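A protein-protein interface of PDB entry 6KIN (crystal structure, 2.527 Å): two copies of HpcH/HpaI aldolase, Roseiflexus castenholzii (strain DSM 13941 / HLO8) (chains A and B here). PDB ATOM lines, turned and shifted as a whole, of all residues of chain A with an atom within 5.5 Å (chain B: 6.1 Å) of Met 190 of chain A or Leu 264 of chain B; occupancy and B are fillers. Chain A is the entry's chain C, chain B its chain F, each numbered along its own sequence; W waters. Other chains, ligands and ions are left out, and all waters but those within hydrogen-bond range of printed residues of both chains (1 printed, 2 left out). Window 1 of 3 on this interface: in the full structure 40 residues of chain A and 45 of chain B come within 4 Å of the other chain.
The backbone NH of Met 190 of chain A is in hydrogen-bond range of the backbone carbonyl oxygen of Ala 185 of chain A (2.9 Å). NZ of Lys 191 of chain A sits at hydrogen-bond distance from O of Gly 189 of chain A (2.7 Å). A ring nitrogen (ND1) of His 199 of chain A lies within hydrogen-bond range of the backbone NH (N) of Phe 201 of chain A (3.0 Å).
Hydrophobic or aromatic side chains of chain B within 4 Å of the printed part of chain A: Phe 263, Leu 264, Leu 265, Val 326 and Ile 327. Hydrophobic or aromatic side chains of chain A that line the printed part of chain B: Ala 185, Ala 186, Met 190, His 199, Phe 201, Tyr 202 and Leu 222. Among the printed residues, no Asp or Glu carboxylate lies within 4 Å of a Lys or Arg side-chain nitrogen of the other chain.
Water W1 lies within hydrogen-bond range of O of Phe 201 of chain A (2.6 Å), OD1 of Asn 261 of chain B (3.0 Å) and NH2 of Arg 260 of chain B (3.3 Å).
Among the printed residues, merely in contact across the chains: Tyr 202 of chain A with Asn 261 of chain B (3.2 Å), Met 190 of chain A with Leu 264 of chain B (3.2 Å), Lys 191 of chain A with Phe 263 of chain B (3.4 Å), Phe 201 of chain A with Leu 264 of chain B (3.5 Å), Thr 192 of chain A with Glu 291 of chain B (3.5 Å), Leu 222 of chain A with Leu 265 of chain B (3.5 Å), Met 190 of chain A with Leu 265 of chain B (3.6 Å), Tyr 202 of chain A with Leu 265 of chain B (3.6 Å), His 199 of chain A with Leu 264 of chain B (3.6 Å), Ala 185 of chain A with Gln 323 of chain B (3.6 Å), Phe 201 of chain A with Arg 260 of chain B (3.6 Å), Gly 189 of chain A with Gly 266 of chain B (3.7 Å), Thr 192 of chain A with Ile 327 of chain B (3.7 Å), Tyr 202 of chain A with Leu 264 of chain B (3.7 Å), Ala 186 of chain A with Val 326 of chain B (3.8 Å) and Ala 186 of chain A with Gln 323 of chain B (3.9 Å).
The backbone carbonyl oxygen (O) of Thr 192 of chain A is in hydrogen-bond range of the side-chain amide nitrogen (NE2) of Gln 323 of chain B (2.7 Å). A ring nitrogen (NE2) of His 199 of chain A lies within hydrogen-bond range of the side-chain carboxylate (OE1) of Glu 291 of chain B (3.4 Å). The backbone carbonyl oxygen of Leu 264 of chain B is in hydrogen-bond range of the backbone NH of Lys 191 of chain A (3.0 Å). The side-chain amide oxygen (OD1) of Asn 261 of chain B sits close to the backbone carbonyl oxygen (O) of Phe 201 of chain A, at 3.3 Å.
No position is printed for both chains. Of the 20 pairs that touch across the chains among the printed residues, none has its exchanged pair printed and touching as well.
Of chain B, only Leu 264 and Leu 265 come within 4 Å of Met 190 of chain A. Leu 264 of chain B touches just these residues of chain A: Met 190, Lys 191, His 199, Phe 201 and Tyr 202. Printed residues of chain B within 4 Å of Thr 192 of chain A: Glu 291, Gln 323 and Ile 327. Of the printed residues of chain A, Phe 263 of chain B touches Lys 191 (3.4 Å). Printed residues of chain B within 4 Å of Leu 222 of chain A: Leu 265 (3.5 Å). Of the printed residues of chain A, Gln 323 of chain B touches Ala 185 (3.6 Å), Ala 186 (3.9 Å) and Thr 192 (2.7 Å). Cys 267 of chain B touches none of the printed residues of chain A. Ala 262 of chain B touches none of the printed residues of chain A. The nearest residue of chain B that does not touch Met 190 of chain A is Gly 266 of chain B (4.4 Å). The nearest residue of chain A that does not touch Leu 264 of chain B is Gly 189 of chain A (4.7 Å). The nearest printed residue of chain B that does not touch Leu 222 of chain A is Leu 264 of chain B (5.0 Å).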
ATOM      1  N   LEU A 184      30.404  -9.229   0.411  1.00  0.00           N
ATOM      2  CA  LEU A 184      29.193  -9.441  -0.366  1.00  0.00           C
ATOM      3  C   LEU A 184      28.052  -8.559   0.132  1.00  0.00           C
ATOM      4  O   LEU A 184      27.245  -8.072  -0.672  1.00  0.00           O
ATOM      5  CB  LEU A 184      28.790 -10.914  -0.348  1.00  0.00           C
ATOM      6  CG  LEU A 184      27.625 -11.193  -1.292  1.00  0.00           C
ATOM      7  CD1 LEU A 184      27.948 -10.752  -2.712  1.00  0.00           C
ATOM      8  CD2 LEU A 184      27.196 -12.658  -1.252  1.00  0.00           C
ATOM      9  N   ALA A 185      27.986  -8.309   1.442  1.00  0.00           N
ATOM     10  CA  ALA A 185      26.989  -7.370   1.951  1.00  0.00           C
ATOM     11  C   ALA A 185      27.268  -5.950   1.476  1.00  0.00           C
ATOM     12  O   ALA A 185      26.340  -5.239   1.076  1.00  0.00           O
ATOM     13  CB  ALA A 185      26.924  -7.422   3.476  1.00  0.00           C
ATOM     14  N   ALA A 186      28.528  -5.509   1.522  1.00  0.00           N
ATOM     15  CA  ALA A 186      28.842  -4.163   1.047  1.00  0.00           C
ATOM     16  C   ALA A 186      28.524  -4.023  -0.432  1.00  0.00           C
ATOM     17  O   ALA A 186      27.987  -2.999  -0.864  1.00  0.00           O
ATOM     18  CB  ALA A 186      30.308  -3.834   1.305  1.00  0.00           C
ATOM     19  N   ARG A 188      26.251  -5.684  -2.186  1.00  0.00           N
ATOM     20  CA  ARG A 188      24.817  -5.698  -2.424  1.00  0.00           C
ATOM     21  C   ARG A 188      24.114  -4.498  -1.837  1.00  0.00           C
ATOM     22  O   ARG A 188      22.955  -4.253  -2.194  1.00  0.00           O
ATOM     23  CB  ARG A 188      24.169  -6.936  -1.815  1.00  0.00           C
ATOM     24  CG  ARG A 188      24.475  -8.269  -2.454  1.00  0.00           C
ATOM     25  CD  ARG A 188      23.987  -9.390  -1.554  1.00  0.00           C
ATOM     26  NE  ARG A 188      23.868 -10.628  -2.299  1.00  0.00           N
ATOM     27  CZ  ARG A 188      23.858 -11.838  -1.756  1.00  0.00           C
ATOM     28  NH1 ARG A 188      23.972 -11.983  -0.444  1.00  0.00           N
ATOM     29  NH2 ARG A 188      23.749 -12.910  -2.535  1.00  0.00           N
ATOM     30  N   GLY A 189      24.774  -3.772  -0.932  1.00  0.00           N
ATOM     31  CA  GLY A 189      24.112  -2.807  -0.080  1.00  0.00           C
ATOM     32  C   GLY A 189      23.256  -3.411   1.022  1.00  0.00           C
ATOM     33  O   GLY A 189      22.311  -2.761   1.471  1.00  0.00           O
ATOM     34  N   MET A 190      23.531  -4.648   1.452  1.00  0.00           N
ATOM     35  CA  MET A 190      22.854  -5.181   2.629  1.00  0.00           C
ATOM     36  C   MET A 190      23.168  -4.295   3.819  1.00  0.00           C
ATOM     37  O   MET A 190      24.300  -3.840   3.984  1.00  0.00           O
ATOM     38  CB  MET A 190      23.302  -6.606   2.944  1.00  0.00           C
ATOM     39  CG  MET A 190      22.723  -7.669   2.074  1.00  0.00           C
ATOM     40  SD  MET A 190      23.658  -9.185   2.337  1.00  0.00           S
ATOM     41  CE  MET A 190      22.509 -10.136   3.337  1.00  0.00           C
ATOM     42  N   LYS A 191      22.172  -4.054   4.661  1.00  0.00           N
ATOM     43  CA  LYS A 191      22.287  -2.981   5.646  1.00  0.00           C
ATOM     44  C   LYS A 191      22.708  -3.545   6.998  1.00  0.00           C
ATOM     45  O   LYS A 191      21.947  -3.639   7.944  1.00  0.00           O
ATOM     46  CB  LYS A 191      20.980  -2.209   5.735  1.00  0.00           C
ATOM     47  CG  LYS A 191      21.089  -0.887   5.082  1.00  0.00           C
ATOM     48  CD  LYS A 191      20.912  -1.046   3.624  1.00  0.00           C
ATOM     49  CE  LYS A 191      21.481   0.128   2.829  1.00  0.00           C
ATOM     50  NZ  LYS A 191      21.318  -0.215   1.381  1.00  0.00           N
ATOM     51  N   THR A 192      23.976  -3.903   7.066  1.00  0.00           N
ATOM     52  CA  THR A 192      24.498  -4.530   8.263  1.00  0.00           C
ATOM     53  C   THR A 192      25.997  -4.379   8.226  1.00  0.00           C
ATOM     54  O   THR A 192      26.596  -4.323   7.144  1.00  0.00           O
ATOM     55  CB  THR A 192      24.135  -6.019   8.373  1.00  0.00           C
ATOM     56  OG1 THR A 192      24.743  -6.561   9.554  1.00  0.00           O
ATOM     57  CG2 THR A 192      24.652  -6.793   7.172  1.00  0.00           C
ATOM     58  N   HIS A 199      20.512 -11.469  12.133  1.00  0.00           N
ATOM     59  CA  HIS A 199      20.363 -10.070  12.418  1.00  0.00           C
ATOM     60  C   HIS A 199      19.057  -9.916  13.186  1.00  0.00           C
ATOM     61  O   HIS A 199      18.044 -10.510  12.794  1.00  0.00           O
ATOM     62  CB  HIS A 199      20.343  -9.210  11.148  1.00  0.00           C
ATOM     63  CG  HIS A 199      20.545  -7.748  11.415  1.00  0.00           C
ATOM     64  ND1 HIS A 199      19.565  -6.953  11.973  1.00  0.00           N
ATOM     65  CD2 HIS A 199      21.619  -6.945  11.223  1.00  0.00           C
ATOM     66  CE1 HIS A 199      20.025  -5.720  12.098  1.00  0.00           C
ATOM     67  NE2 HIS A 199      21.270  -5.688  11.651  1.00  0.00           N
ATOM     68  N   PHE A 201      16.939  -7.570  13.199  1.00  0.00           N
ATOM     69  CA  PHE A 201      15.884  -6.945  12.411  1.00  0.00           C
ATOM     70  C   PHE A 201      15.350  -7.809  11.276  1.00  0.00           C
ATOM     71  O   PHE A 201      14.362  -7.404  10.651  1.00  0.00           O
ATOM     72  CB  PHE A 201      16.362  -5.619  11.804  1.00  0.00           C
ATOM     73  CG  PHE A 201      16.679  -4.557  12.819  1.00  0.00           C
ATOM     74  CD1 PHE A 201      16.217  -4.661  14.130  1.00  0.00           C
ATOM     75  CD2 PHE A 201      17.445  -3.451  12.462  1.00  0.00           C
ATOM     76  CE1 PHE A 201      16.519  -3.687  15.067  1.00  0.00           C
ATOM     77  CE2 PHE A 201      17.751  -2.463  13.401  1.00  0.00           C
ATOM     78  CZ  PHE A 201      17.288  -2.584  14.702  1.00  0.00           C
ATOM     79  N   TYR A 202      15.969  -8.960  10.962  1.00  0.00           N
ATOM     80  CA  TYR A 202      15.511  -9.800   9.854  1.00  0.00           C
ATOM     81  C   TYR A 202      14.662 -10.955  10.409  1.00  0.00           C
ATOM     82  O   TYR A 202      15.189 -11.989  10.826  1.00  0.00           O
ATOM     83  CB  TYR A 202      16.690 -10.305   9.018  1.00  0.00           C
ATOM     84  CG  TYR A 202      16.250 -10.999   7.732  1.00  0.00           C
ATOM     85  CD1 TYR A 202      15.392 -10.354   6.845  1.00  0.00           C
ATOM     86  CD2 TYR A 202      16.666 -12.299   7.416  1.00  0.00           C
ATOM     87  CE1 TYR A 202      14.960 -10.962   5.687  1.00  0.00           C
ATOM     88  CE2 TYR A 202      16.239 -12.922   6.236  1.00  0.00           C
ATOM     89  CZ  TYR A 202      15.382 -12.239   5.377  1.00  0.00           C
ATOM     90  OH  TYR A 202      14.905 -12.797   4.207  1.00  0.00           O
ATOM     91  N   LEU A 222      19.746 -14.806   6.923  1.00  0.00           N
ATOM     92  CA  LEU A 222      20.123 -13.858   5.881  1.00  0.00           C
ATOM     93  C   LEU A 222      20.713 -14.545   4.657  1.00  0.00           C
ATOM     94  O   LEU A 222      20.548 -14.054   3.541  1.00  0.00           O
ATOM     95  CB  LEU A 222      21.143 -12.856   6.414  1.00  0.00           C
ATOM     96  CG  LEU A 222      20.555 -11.567   6.981  1.00  0.00           C
ATOM     97  CD1 LEU A 222      21.668 -10.575   7.304  1.00  0.00           C
ATOM     98  CD2 LEU A 222      19.567 -10.975   5.982  1.00  0.00           C
ATOM     99  N   TRP A 223      21.416 -15.662   4.845  1.00  0.00           N
ATOM    100  CA  TRP A 223      22.285 -16.193   3.809  1.00  0.00           C
ATOM    101  C   TRP A 223      21.753 -17.472   3.184  1.00  0.00           C
ATOM    102  O   TRP A 223      22.509 -18.187   2.528  1.00  0.00           O
ATOM    103  CB  TRP A 223      23.692 -16.422   4.367  1.00  0.00           C
ATOM    104  CG  TRP A 223      24.256 -15.188   4.985  1.00  0.00           C
ATOM    105  CD1 TRP A 223      24.286 -14.870   6.315  1.00  0.00           C
ATOM    106  CD2 TRP A 223      24.843 -14.083   4.297  1.00  0.00           C
ATOM    107  NE1 TRP A 223      24.861 -13.629   6.494  1.00  0.00           N
ATOM    108  CE2 TRP A 223      25.213 -13.130   5.270  1.00  0.00           C
ATOM    109  CE3 TRP A 223      25.101 -13.808   2.951  1.00  0.00           C
ATOM    110  CZ2 TRP A 223      25.822 -11.945   4.943  1.00  0.00           C
ATOM    111  CZ3 TRP A 223      25.705 -12.619   2.627  1.00  0.00           C
ATOM    112  CH2 TRP A 223      26.064 -11.705   3.615  1.00  0.00           C
ATOM    113  N   PHE B 259       8.831  -4.256   5.723  1.00  0.00           N
ATOM    114  CA  PHE B 259       9.685  -3.234   5.125  1.00  0.00           C
ATOM    115  C   PHE B 259      11.132  -3.376   5.584  1.00  0.00           C
ATOM    116  O   PHE B 259      12.053  -3.230   4.772  1.00  0.00           O
ATOM    117  CB  PHE B 259       9.164  -1.832   5.448  1.00  0.00           C
ATOM    118  CG  PHE B 259       8.010  -1.396   4.590  1.00  0.00           C
ATOM    119  CD1 PHE B 259       7.464  -2.245   3.646  1.00  0.00           C
ATOM    120  CD2 PHE B 259       7.475  -0.134   4.723  1.00  0.00           C
ATOM    121  CE1 PHE B 259       6.400  -1.840   2.856  1.00  0.00           C
ATOM    122  CE2 PHE B 259       6.414   0.263   3.945  1.00  0.00           C
ATOM    123  CZ  PHE B 259       5.879  -0.592   3.007  1.00  0.00           C
ATOM    124  N   ARG B 260      11.356  -3.678   6.875  1.00  0.00           N
ATOM    125  CA  ARG B 260      12.726  -3.727   7.388  1.00  0.00           C
ATOM    126  C   ARG B 260      13.486  -4.927   6.828  1.00  0.00           C
ATOM    127  O   ARG B 260      14.688  -4.837   6.556  1.00  0.00           O
ATOM    128  CB  ARG B 260      12.727  -3.730   8.918  1.00  0.00           C
ATOM    129  CG  ARG B 260      13.938  -3.005   9.540  1.00  0.00           C
ATOM    130  CD  ARG B 260      13.913  -2.954  11.085  1.00  0.00           C
ATOM    131  NE  ARG B 260      13.077  -4.023  11.628  1.00  0.00           N
ATOM    132  CZ  ARG B 260      11.951  -3.807  12.305  1.00  0.00           C
ATOM    133  NH1 ARG B 260      11.546  -2.558  12.528  1.00  0.00           N
ATOM    134  NH2 ARG B 260      11.231  -4.835  12.745  1.00  0.00           N
ATOM    135  N   ASN B 261      12.807  -6.053   6.638  1.00  0.00           N
ATOM    136  CA  ASN B 261      13.434  -7.170   5.943  1.00  0.00           C
ATOM    137  C   ASN B 261      13.924  -6.737   4.567  1.00  0.00           C
ATOM    138  O   ASN B 261      15.111  -6.873   4.240  1.00  0.00           O
ATOM    139  CB  ASN B 261      12.453  -8.329   5.822  1.00  0.00           C
ATOM    140  CG  ASN B 261      12.103  -8.919   7.155  1.00  0.00           C
ATOM    141  OD1 ASN B 261      12.870  -8.820   8.119  1.00  0.00           O
ATOM    142  ND2 ASN B 261      10.940  -9.545   7.225  1.00  0.00           N
ATOM    143  N   ALA B 262      13.017  -6.185   3.757  1.00  0.00           N
ATOM    144  CA  ALA B 262      13.398  -5.658   2.453  1.00  0.00           C
ATOM    145  C   ALA B 262      14.617  -4.751   2.567  1.00  0.00           C
ATOM    146  O   ALA B 262      15.592  -4.908   1.824  1.00  0.00           O
ATOM    147  CB  ALA B 262      12.214  -4.913   1.822  1.00  0.00           C
ATOM    148  N   PHE B 263      14.592  -3.816   3.518  1.00  0.00           N
ATOM    149  CA  PHE B 263      15.714  -2.890   3.674  1.00  0.00           C
ATOM    150  C   PHE B 263      16.999  -3.637   3.990  1.00  0.00           C
ATOM    151  O   PHE B 263      18.070  -3.283   3.485  1.00  0.00           O
ATOM    152  CB  PHE B 263      15.410  -1.874   4.775  1.00  0.00           C
ATOM    153  CG  PHE B 263      16.485  -0.853   5.007  1.00  0.00           C
ATOM    154  CD1 PHE B 263      16.866   0.030   4.006  1.00  0.00           C
ATOM    155  CD2 PHE B 263      17.074  -0.730   6.254  1.00  0.00           C
ATOM    156  CE1 PHE B 263      17.843   1.005   4.231  1.00  0.00           C
ATOM    157  CE2 PHE B 263      18.049   0.253   6.496  1.00  0.00           C
ATOM    158  CZ  PHE B 263      18.430   1.117   5.480  1.00  0.00           C
ATOM    159  N   LEU B 264      16.914  -4.675   4.824  1.00  0.00           N
ATOM    160  CA  LEU B 264      18.136  -5.340   5.239  1.00  0.00           C
ATOM    161  C   LEU B 264      18.784  -6.069   4.068  1.00  0.00           C
ATOM    162  O   LEU B 264      20.011  -6.040   3.925  1.00  0.00           O
ATOM    163  CB  LEU B 264      17.859  -6.285   6.400  1.00  0.00           C
ATOM    164  CG  LEU B 264      17.663  -5.561   7.727  1.00  0.00           C
ATOM    165  CD1 LEU B 264      17.883  -6.565   8.828  1.00  0.00           C
ATOM    166  CD2 LEU B 264      18.620  -4.388   7.881  1.00  0.00           C
ATOM    167  N   LEU B 265      17.972  -6.675   3.194  1.00  0.00           N
ATOM    168  CA  LEU B 265      18.513  -7.432   2.072  1.00  0.00           C
ATOM    169  C   LEU B 265      19.075  -6.533   0.978  1.00  0.00           C
ATOM    170  O   LEU B 265      19.818  -7.021   0.122  1.00  0.00           O
ATOM    171  CB  LEU B 265      17.442  -8.370   1.510  1.00  0.00           C
ATOM    172  CG  LEU B 265      17.064  -9.578   2.394  1.00  0.00           C
ATOM    173  CD1 LEU B 265      15.987 -10.457   1.744  1.00  0.00           C
ATOM    174  CD2 LEU B 265      18.282 -10.419   2.736  1.00  0.00           C
ATOM    175  N   GLY B 266      18.780  -5.233   1.003  1.00  0.00           N
ATOM    176  CA  GLY B 266      19.319  -4.312   0.019  1.00  0.00           C
ATOM    177  C   GLY B 266      18.294  -3.522  -0.777  1.00  0.00           C
ATOM    178  O   GLY B 266      18.668  -2.795  -1.697  1.00  0.00           O
ATOM    179  N   CYS B 267      17.008  -3.631  -0.453  1.00  0.00           N
ATOM    180  CA  CYS B 267      16.015  -2.791  -1.114  1.00  0.00           C
ATOM    181  C   CYS B 267      16.190  -1.341  -0.697  1.00  0.00           C
ATOM    182  O   CYS B 267      16.616  -1.048   0.424  1.00  0.00           O
ATOM    183  CB  CYS B 267      14.601  -3.248  -0.782  1.00  0.00           C
ATOM    184  SG  CYS B 267      14.206  -4.829  -1.543  1.00  0.00           S
ATOM    185  N   GLU B 291      22.870   1.496  14.521  1.00  0.00           N
ATOM    186  CA  GLU B 291      23.685   0.945  13.443  1.00  0.00           C
ATOM    187  C   GLU B 291      24.561   2.012  12.782  1.00  0.00           C
ATOM    188  O   GLU B 291      25.710   1.728  12.407  1.00  0.00           O
ATOM    189  CB  GLU B 291      22.777   0.260  12.423  1.00  0.00           C
ATOM    190  CG  GLU B 291      23.513  -0.588  11.422  1.00  0.00           C
ATOM    191  CD  GLU B 291      23.366  -2.085  11.699  1.00  0.00           C
ATOM    192  OE1 GLU B 291      22.304  -2.479  12.254  1.00  0.00           O
ATOM    193  OE2 GLU B 291      24.304  -2.861  11.345  1.00  0.00           O
ATOM    194  N   GLN B 323      31.391  -1.849   4.450  1.00  0.00           N
ATOM    195  CA  GLN B 323      30.040  -1.961   4.983  1.00  0.00           C
ATOM    196  C   GLN B 323      29.648  -0.685   5.718  1.00  0.00           C
ATOM    197  O   GLN B 323      28.558  -0.137   5.502  1.00  0.00           O
ATOM    198  CB  GLN B 323      29.935  -3.181   5.905  1.00  0.00           C
ATOM    199  CG  GLN B 323      29.750  -4.497   5.174  1.00  0.00           C
ATOM    200  CD  GLN B 323      29.705  -5.692   6.116  1.00  0.00           C
ATOM    201  OE1 GLN B 323      30.740  -6.214   6.523  1.00  0.00           O
ATOM    202  NE2 GLN B 323      28.505  -6.132   6.463  1.00  0.00           N
ATOM    203  N   VAL B 326      28.910   2.275   3.285  1.00  0.00           N
ATOM    204  CA  VAL B 326      27.536   2.199   2.791  1.00  0.00           C
ATOM    205  C   VAL B 326      26.571   2.792   3.820  1.00  0.00           C
ATOM    206  O   VAL B 326      25.789   3.708   3.521  1.00  0.00           O
ATOM    207  CB  VAL B 326      27.161   0.743   2.452  1.00  0.00           C
ATOM    208  CG1 VAL B 326      25.660   0.633   2.143  1.00  0.00           C
ATOM    209  CG2 VAL B 326      28.049   0.172   1.314  1.00  0.00           C
ATOM    210  N   ILE B 327      26.634   2.290   5.055  1.00  0.00           N
ATOM    211  CA  ILE B 327      25.666   2.690   6.069  1.00  0.00           C
ATOM    212  C   ILE B 327      25.795   4.179   6.385  1.00  0.00           C
ATOM    213  O   ILE B 327      24.799   4.908   6.396  1.00  0.00           O
ATOM    214  CB  ILE B 327      25.808   1.802   7.321  1.00  0.00           C
ATOM    215  CG1 ILE B 327      25.080   0.469   7.088  1.00  0.00           C
ATOM    216  CG2 ILE B 327      25.219   2.483   8.533  1.00  0.00           C
ATOM    217  CD1 ILE B 327      25.585  -0.677   7.908  1.00  0.00           C
HETATM  218  O   HOH W   1      11.804  -7.051  10.302  1.00  0.00           O
